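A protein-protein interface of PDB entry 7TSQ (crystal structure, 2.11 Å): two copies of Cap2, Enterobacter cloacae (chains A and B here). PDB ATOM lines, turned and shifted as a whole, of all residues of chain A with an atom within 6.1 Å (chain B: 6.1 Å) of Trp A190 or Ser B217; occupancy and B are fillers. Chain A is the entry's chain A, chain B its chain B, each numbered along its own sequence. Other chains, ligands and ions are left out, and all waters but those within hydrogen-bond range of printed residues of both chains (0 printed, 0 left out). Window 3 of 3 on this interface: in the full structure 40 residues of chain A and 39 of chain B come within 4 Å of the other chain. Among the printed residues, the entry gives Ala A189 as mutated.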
ATOM      1  N   GLY A 188      24.771  19.223  -7.694  1.00  0.00           N
ATOM      2  CA  GLY A 188      23.941  18.677  -8.745  1.00  0.00           C
ATOM      3  C   GLY A 188      23.757  17.179  -8.635  1.00  0.00           C
ATOM      4  O   GLY A 188      24.108  16.588  -7.624  1.00  0.00           O
ATOM      5  N   ALA A 189      23.179  16.572  -9.670  1.00  0.00           N
ATOM      6  CA  ALA A 189      23.017  15.126  -9.696  1.00  0.00           C
ATOM      7  C   ALA A 189      24.338  14.382  -9.813  1.00  0.00           C
ATOM      8  O   ALA A 189      24.371  13.171  -9.568  1.00  0.00           O
ATOM      9  CB  ALA A 189      22.106  14.720 -10.843  1.00  0.00           C
ATOM     10  N   TRP A 190      25.427  15.086 -10.131  1.00  0.00           N
ATOM     11  CA  TRP A 190      26.745  14.470 -10.149  1.00  0.00           C
ATOM     12  C   TRP A 190      27.152  13.949  -8.776  1.00  0.00           C
ATOM     13  O   TRP A 190      27.938  13.004  -8.687  1.00  0.00           O
ATOM     14  CB  TRP A 190      27.780  15.474 -10.663  1.00  0.00           C
ATOM     15  CG  TRP A 190      27.712  16.817  -9.957  1.00  0.00           C
ATOM     16  CD1 TRP A 190      27.078  17.949 -10.390  1.00  0.00           C
ATOM     17  CD2 TRP A 190      28.293  17.148  -8.691  1.00  0.00           C
ATOM     18  NE1 TRP A 190      27.226  18.960  -9.470  1.00  0.00           N
ATOM     19  CE2 TRP A 190      27.969  18.491  -8.417  1.00  0.00           C
ATOM     20  CE3 TRP A 190      29.054  16.436  -7.760  1.00  0.00           C
ATOM     21  CZ2 TRP A 190      28.385  19.137  -7.254  1.00  0.00           C
ATOM     22  CZ3 TRP A 190      29.465  17.079  -6.607  1.00  0.00           C
ATOM     23  CH2 TRP A 190      29.130  18.415  -6.363  1.00  0.00           C
ATOM     24  N   HIS A 191      26.629  14.541  -7.705  1.00  0.00           N
ATOM     25  CA  HIS A 191      27.009  14.134  -6.355  1.00  0.00           C
ATOM     26  C   HIS A 191      26.634  12.675  -6.131  1.00  0.00           C
ATOM     27  O   HIS A 191      25.519  12.263  -6.486  1.00  0.00           O
ATOM     28  CB  HIS A 191      26.307  15.022  -5.328  1.00  0.00           C
ATOM     29  CG  HIS A 191      26.973  15.044  -3.985  1.00  0.00           C
ATOM     30  ND1 HIS A 191      26.851  14.021  -3.067  1.00  0.00           N
ATOM     31  CD2 HIS A 191      27.755  15.982  -3.399  1.00  0.00           C
ATOM     32  CE1 HIS A 191      27.539  14.324  -1.981  1.00  0.00           C
ATOM     33  NE2 HIS A 191      28.098  15.508  -2.155  1.00  0.00           N
ATOM     34  N   PRO A 192      27.523  11.858  -5.548  1.00  0.00           N
ATOM     35  CA  PRO A 192      27.220  10.420  -5.441  1.00  0.00           C
ATOM     36  C   PRO A 192      25.939  10.102  -4.690  1.00  0.00           C
ATOM     37  O   PRO A 192      25.326   9.066  -4.967  1.00  0.00           O
ATOM     38  CB  PRO A 192      28.454   9.854  -4.725  1.00  0.00           C
ATOM     39  CG  PRO A 192      29.567  10.831  -5.035  1.00  0.00           C
ATOM     40  CD  PRO A 192      28.886  12.184  -5.080  1.00  0.00           C
ATOM     41  N   VAL A 193      25.490  10.967  -3.779  1.00  0.00           N
ATOM     42  CA  VAL A 193      24.306  10.667  -2.984  1.00  0.00           C
ATOM     43  C   VAL A 193      23.047  10.665  -3.842  1.00  0.00           C
ATOM     44  O   VAL A 193      22.073   9.982  -3.515  1.00  0.00           O
ATOM     45  CB  VAL A 193      24.203  11.668  -1.815  1.00  0.00           C
ATOM     46  CG1 VAL A 193      23.802  13.052  -2.325  1.00  0.00           C
ATOM     47  CG2 VAL A 193      23.242  11.181  -0.745  1.00  0.00           C
ATOM     48  N   PHE A 194      23.044  11.414  -4.949  1.00  0.00           N
ATOM     49  CA  PHE A 194      21.890  11.494  -5.839  1.00  0.00           C
ATOM     50  C   PHE A 194      21.692  10.163  -6.571  1.00  0.00           C
ATOM     51  O   PHE A 194      22.548   9.278  -6.511  1.00  0.00           O
ATOM     52  CB  PHE A 194      22.073  12.631  -6.851  1.00  0.00           C
ATOM     53  CG  PHE A 194      21.712  14.010  -6.312  1.00  0.00           C
ATOM     54  CD1 PHE A 194      22.503  14.653  -5.363  1.00  0.00           C
ATOM     55  CD2 PHE A 194      20.586  14.673  -6.781  1.00  0.00           C
ATOM     56  CE1 PHE A 194      22.160  15.915  -4.882  1.00  0.00           C
ATOM     57  CE2 PHE A 194      20.240  15.932  -6.308  1.00  0.00           C
ATOM     58  CZ  PHE A 194      21.028  16.553  -5.358  1.00  0.00           C
ATOM     59  N   ARG A 197      23.276   7.671 -12.458  1.00  0.00           N
ATOM     60  CA  ARG A 197      23.220   8.137 -13.840  1.00  0.00           C
ATOM     61  C   ARG A 197      24.143   7.270 -14.688  1.00  0.00           C
ATOM     62  O   ARG A 197      24.795   6.354 -14.186  1.00  0.00           O
ATOM     63  CB  ARG A 197      23.606   9.618 -13.943  1.00  0.00           C
ATOM     64  CG  ARG A 197      22.810  10.543 -13.021  1.00  0.00           C
ATOM     65  CD  ARG A 197      23.139  12.016 -13.268  1.00  0.00           C
ATOM     66  NE  ARG A 197      24.568  12.297 -13.149  1.00  0.00           N
ATOM     67  CZ  ARG A 197      25.121  13.480 -13.369  1.00  0.00           C
ATOM     68  NH1 ARG A 197      24.395  14.534 -13.705  1.00  0.00           N
ATOM     69  NH2 ARG A 197      26.442  13.611 -13.254  1.00  0.00           N
ATOM     70  N   ASP A 199      26.994   8.051 -16.012  1.00  0.00           N
ATOM     71  CA  ASP A 199      28.404   8.170 -15.662  1.00  0.00           C
ATOM     72  C   ASP A 199      28.735   7.421 -14.380  1.00  0.00           C
ATOM     73  O   ASP A 199      29.836   6.861 -14.269  1.00  0.00           O
ATOM     74  CB  ASP A 199      28.847   9.635 -15.581  1.00  0.00           C
ATOM     75  CG  ASP A 199      28.023  10.490 -14.624  1.00  0.00           C
ATOM     76  OD1 ASP A 199      27.002  10.016 -14.085  1.00  0.00           O
ATOM     77  OD2 ASP A 199      28.419  11.663 -14.414  1.00  0.00           O
ATOM     78  N   ASP A 200      27.794   7.325 -13.429  1.00  0.00           N
ATOM     79  CA  ASP A 200      28.017   6.525 -12.234  1.00  0.00           C
ATOM     80  C   ASP A 200      28.212   5.058 -12.580  1.00  0.00           C
ATOM     81  O   ASP A 200      29.122   4.398 -12.074  1.00  0.00           O
ATOM     82  CB  ASP A 200      26.857   6.669 -11.254  1.00  0.00           C
ATOM     83  CG  ASP A 200      26.709   8.080 -10.695  1.00  0.00           C
ATOM     84  OD1 ASP A 200      27.572   8.534  -9.909  1.00  0.00           O
ATOM     85  OD2 ASP A 200      25.712   8.743 -11.049  1.00  0.00           O
ATOM     86  N   GLN A 228      32.696   6.212  -4.363  1.00  0.00           N
ATOM     87  CA  GLN A 228      32.773   7.487  -5.085  1.00  0.00           C
ATOM     88  C   GLN A 228      32.658   8.646  -4.100  1.00  0.00           C
ATOM     89  O   GLN A 228      31.854   8.600  -3.168  1.00  0.00           O
ATOM     90  CB  GLN A 228      31.644   7.584  -6.115  1.00  0.00           C
ATOM     91  CG  GLN A 228      31.836   8.635  -7.223  1.00  0.00           C
ATOM     92  CD  GLN A 228      30.621   8.765  -8.155  1.00  0.00           C
ATOM     93  OE1 GLN A 228      30.369   9.828  -8.733  1.00  0.00           O
ATOM     94  NE2 GLN A 228      29.862   7.682  -8.298  1.00  0.00           N
ATOM     95  N   PRO A 230      32.573  13.110  -3.445  1.00  0.00           N
ATOM     96  CA  PRO A 230      32.012  14.277  -4.156  1.00  0.00           C
ATOM     97  C   PRO A 230      33.032  15.042  -4.981  1.00  0.00           C
ATOM     98  O   PRO A 230      32.656  15.696  -5.963  1.00  0.00           O
ATOM     99  CB  PRO A 230      31.434  15.145  -3.027  1.00  0.00           C
ATOM    100  CG  PRO A 230      31.208  14.188  -1.872  1.00  0.00           C
ATOM    101  CD  PRO A 230      32.354  13.192  -1.986  1.00  0.00           C
ATOM    102  N   ASP A 231      34.314  14.964  -4.628  1.00  0.00           N
ATOM    103  CA  ASP A 231      35.344  15.678  -5.370  1.00  0.00           C
ATOM    104  C   ASP A 231      35.824  14.928  -6.604  1.00  0.00           C
ATOM    105  O   ASP A 231      36.731  15.417  -7.286  1.00  0.00           O
ATOM    106  CB  ASP A 231      36.535  16.005  -4.456  1.00  0.00           C
ATOM    107  CG  ASP A 231      37.242  14.758  -3.916  1.00  0.00           C
ATOM    108  OD1 ASP A 231      36.616  13.679  -3.837  1.00  0.00           O
ATOM    109  OD2 ASP A 231      38.437  14.875  -3.553  1.00  0.00           O
ATOM    110  N   ASN B  15      21.775  26.423 -14.010  1.00  0.00           N
ATOM    111  CA  ASN B  15      22.897  25.623 -13.545  1.00  0.00           C
ATOM    112  C   ASN B  15      22.844  24.174 -14.033  1.00  0.00           C
ATOM    113  O   ASN B  15      23.641  23.352 -13.574  1.00  0.00           O
ATOM    114  CB  ASN B  15      22.966  25.664 -12.011  1.00  0.00           C
ATOM    115  CG  ASN B  15      21.684  25.161 -11.338  1.00  0.00           C
ATOM    116  OD1 ASN B  15      20.671  24.934 -11.988  1.00  0.00           O
ATOM    117  ND2 ASN B  15      21.732  24.988 -10.029  1.00  0.00           N
ATOM    118  N   ASP B  16      21.985  23.870 -15.006  1.00  0.00           N
ATOM    119  CA  ASP B  16      21.678  22.500 -15.416  1.00  0.00           C
ATOM    120  C   ASP B  16      22.122  22.277 -16.854  1.00  0.00           C
ATOM    121  O   ASP B  16      21.629  22.935 -17.775  1.00  0.00           O
ATOM    122  CB  ASP B  16      20.173  22.258 -15.283  1.00  0.00           C
ATOM    123  CG  ASP B  16      19.800  20.777 -15.243  1.00  0.00           C
ATOM    124  OD1 ASP B  16      20.682  19.919 -15.436  1.00  0.00           O
ATOM    125  OD2 ASP B  16      18.607  20.475 -15.004  1.00  0.00           O
ATOM    126  N   ILE B  17      23.031  21.312 -17.055  1.00  0.00           N
ATOM    127  CA  ILE B  17      23.580  21.070 -18.387  1.00  0.00           C
ATOM    128  C   ILE B  17      22.536  20.457 -19.318  1.00  0.00           C
ATOM    129  O   ILE B  17      22.641  20.585 -20.543  1.00  0.00           O
ATOM    130  CB  ILE B  17      24.849  20.193 -18.285  1.00  0.00           C
ATOM    131  CG1 ILE B  17      25.564  20.114 -19.638  1.00  0.00           C
ATOM    132  CG2 ILE B  17      24.510  18.788 -17.810  1.00  0.00           C
ATOM    133  CD1 ILE B  17      26.990  19.556 -19.564  1.00  0.00           C
ATOM    134  N   THR B 209      32.761  13.586 -17.300  1.00  0.00           N
ATOM    135  CA  THR B 209      31.351  13.950 -17.329  1.00  0.00           C
ATOM    136  C   THR B 209      30.884  14.465 -15.978  1.00  0.00           C
ATOM    137  O   THR B 209      30.046  15.372 -15.904  1.00  0.00           O
ATOM    138  CB  THR B 209      30.534  12.740 -17.769  1.00  0.00           C
ATOM    139  OG1 THR B 209      30.909  12.366 -19.099  1.00  0.00           O
ATOM    140  CG2 THR B 209      29.043  13.047 -17.740  1.00  0.00           C
ATOM    141  N   LYS B 210      31.446  13.932 -14.885  1.00  0.00           N
ATOM    142  CA  LYS B 210      31.166  14.474 -13.557  1.00  0.00           C
ATOM    143  C   LYS B 210      31.840  15.825 -13.345  1.00  0.00           C
ATOM    144  O   LYS B 210      31.305  16.699 -12.651  1.00  0.00           O
ATOM    145  CB  LYS B 210      31.596  13.468 -12.484  1.00  0.00           C
ATOM    146  CG  LYS B 210      30.871  12.119 -12.568  1.00  0.00           C
ATOM    147  CD  LYS B 210      31.655  10.978 -11.923  1.00  0.00           C
ATOM    148  CE  LYS B 210      30.990   9.618 -12.160  1.00  0.00           C
ATOM    149  NZ  LYS B 210      29.577   9.595 -11.690  1.00  0.00           N
ATOM    150  N   ILE B 212      32.409  17.921 -15.920  1.00  0.00           N
ATOM    151  CA  ILE B 212      31.632  18.809 -16.774  1.00  0.00           C
ATOM    152  C   ILE B 212      30.367  19.275 -16.066  1.00  0.00           C
ATOM    153  O   ILE B 212      29.966  20.441 -16.162  1.00  0.00           O
ATOM    154  CB  ILE B 212      31.305  18.100 -18.105  1.00  0.00           C
ATOM    155  CG1 ILE B 212      32.557  18.003 -18.980  1.00  0.00           C
ATOM    156  CG2 ILE B 212      30.193  18.827 -18.829  1.00  0.00           C
ATOM    157  CD1 ILE B 212      32.484  16.928 -20.055  1.00  0.00           C
ATOM    158  N   CYS B 213      29.726  18.371 -15.313  1.00  0.00           N
ATOM    159  CA  CYS B 213      28.484  18.715 -14.630  1.00  0.00           C
ATOM    160  C   CYS B 213      28.726  19.577 -13.399  1.00  0.00           C
ATOM    161  O   CYS B 213      27.882  20.410 -13.045  1.00  0.00           O
ATOM    162  CB  CYS B 213      27.738  17.439 -14.248  1.00  0.00           C
ATOM    163  SG  CYS B 213      27.102  16.462 -15.657  1.00  0.00           S
ATOM    164  N   ARG B 214      29.858  19.390 -12.720  1.00  0.00           N
ATOM    165  CA  ARG B 214      30.201  20.275 -11.614  1.00  0.00           C
ATOM    166  C   ARG B 214      30.535  21.684 -12.094  1.00  0.00           C
ATOM    167  O   ARG B 214      30.256  22.661 -11.394  1.00  0.00           O
ATOM    168  CB  ARG B 214      31.372  19.713 -10.810  1.00  0.00           C
ATOM    169  CG  ARG B 214      31.067  18.457  -9.979  1.00  0.00           C
ATOM    170  CD  ARG B 214      32.327  17.602  -9.766  1.00  0.00           C
ATOM    171  NE  ARG B 214      33.373  18.315  -9.039  1.00  0.00           N
ATOM    172  CZ  ARG B 214      34.669  18.063  -9.161  1.00  0.00           C
ATOM    173  NH1 ARG B 214      35.118  17.142  -9.998  1.00  0.00           N
ATOM    174  NH2 ARG B 214      35.538  18.759  -8.429  1.00  0.00           N
ATOM    175  N   VAL B 215      31.107  21.811 -13.296  1.00  0.00           N
ATOM    176  CA  VAL B 215      31.491  23.121 -13.816  1.00  0.00           C
ATOM    177  C   VAL B 215      30.265  23.919 -14.241  1.00  0.00           C
ATOM    178  O   VAL B 215      30.143  25.110 -13.940  1.00  0.00           O
ATOM    179  CB  VAL B 215      32.488  22.958 -14.980  1.00  0.00           C
ATOM    180  CG1 VAL B 215      32.632  24.257 -15.755  1.00  0.00           C
ATOM    181  CG2 VAL B 215      33.834  22.485 -14.460  1.00  0.00           C
ATOM    182  N   VAL B 216      29.330  23.282 -14.955  1.00  0.00           N
ATOM    183  CA  VAL B 216      28.132  23.993 -15.400  1.00  0.00           C
ATOM    184  C   VAL B 216      27.230  24.343 -14.227  1.00  0.00           C
ATOM    185  O   VAL B 216      26.475  25.326 -14.280  1.00  0.00           O
ATOM    186  CB  VAL B 216      27.380  23.153 -16.449  1.00  0.00           C
ATOM    187  CG1 VAL B 216      26.037  23.794 -16.790  1.00  0.00           C
ATOM    188  CG2 VAL B 216      28.229  22.967 -17.701  1.00  0.00           C
ATOM    189  N   SER B 217      27.295  23.565 -13.143  1.00  0.00           N
ATOM    190  CA  SER B 217      26.509  23.864 -11.952  1.00  0.00           C
ATOM    191  C   SER B 217      27.089  25.014 -11.137  1.00  0.00           C
ATOM    192  O   SER B 217      26.349  25.671 -10.402  1.00  0.00           O
ATOM    193  CB  SER B 217      26.388  22.639 -11.055  1.00  0.00           C
ATOM    194  OG  SER B 217      25.646  21.608 -11.671  1.00  0.00           O
ATOM    195  N   ALA B 218      28.384  25.291 -11.291  1.00  0.00           N
ATOM    196  CA  ALA B 218      29.055  26.381 -10.577  1.00  0.00           C
ATOM    197  C   ALA B 218      30.172  26.909 -11.437  1.00  0.00           C
ATOM    198  O   ALA B 218      31.370  26.611 -11.210  1.00  0.00           O
ATOM    199  CB  ALA B 218      29.569  25.915  -9.219  1.00  0.00           C
ATOM    200  N   PRO B 219      29.880  27.718 -12.454  1.00  0.00           N
ATOM    201  CA  PRO B 219      30.901  28.121 -13.417  1.00  0.00           C
ATOM    202  C   PRO B 219      31.981  29.002 -12.796  1.00  0.00           C
ATOM    203  O   PRO B 219      31.715  29.812 -11.902  1.00  0.00           O
ATOM    204  CB  PRO B 219      30.114  28.874 -14.493  1.00  0.00           C
ATOM    205  CG  PRO B 219      28.686  28.299 -14.392  1.00  0.00           C
ATOM    206  CD  PRO B 219      28.502  28.041 -12.907  1.00  0.00           C
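The side-chain carboxylate of Asp A199 lies within salt-bridge range of the side-chain amino group of Lys B210, 3.5 Å away.
OD1 of Asp A200 lies within salt-bridge range of NZ of Lys B210, 2.9 Å away.
The side-chain amino group of Lys B210 lies within hydrogen-bond range of the side-chain amide oxygen of Gln A228, 3.1 Å away.
The guanidinium group (NH2) of Arg A197 is in hydrogen-bond range of the side-chain sulfur (SG) of Cys B213 (3.8 Å).
N of Arg A197 sits at hydrogen-bond distance from OD2 of Asp A200 (3.0 Å).
OG of Ser B217 is in hydrogen-bond range of O of Cys B213, at 2.9 Å.
The backbone carbonyl oxygen of Thr B209 is in hydrogen-bond range of the side-chain sulfur of Cys B213.
O of Asn B15 sits at hydrogen-bond distance from OG of Ser B217.
NH2 of Arg A197 lies within salt-bridge range of OD2 of Asp A199 (3.0 Å).
OD1 of Asp A200 sits at hydrogen-bond distance from NE2 of Gln A228 (2.9 Å).
Among the printed residues, merely in contact across the chains: Trp A190 with Arg B214 (3.3 Å), Asp A231 with Arg B214 (3.6 Å), Asp A199 with Thr B209 (3.7 Å), Trp A190 with Cys B213 (3.7 Å) and Trp A190 with Ser B217 (3.8 Å).
Of chain B, only Cys B213, Arg B214 and Ser B217 come within 4 Å of Trp A190.
Of the printed residues of chain B, Asp A200 touches Lys B210.
Of the printed residues of chain A, Lys B210 touches Asp A199, Asp A200 and Gln A228.
Printed residues of chain A within 4 Å of Arg B214: Trp A190 and Asp A231.
The nearest residue of chain B that does not touch Trp A190 is Lys B210 (4.2 Å).
The nearest residue of chain A that does not touch Ser B217 is Gly A188 (4.5 Å).
Of the 13 printed residues of chain B, 5 touch a printed residue of chain A.
Among the printed residues, 9 pairs touch across the chains.
Among the printed residues, Asp or Glu carboxylates within 4 Å of a Lys or Arg side-chain nitrogen of the other chain: Asp A199 with Lys B210 and Asp A200 with Lys B210.
No position is printed for both chains.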
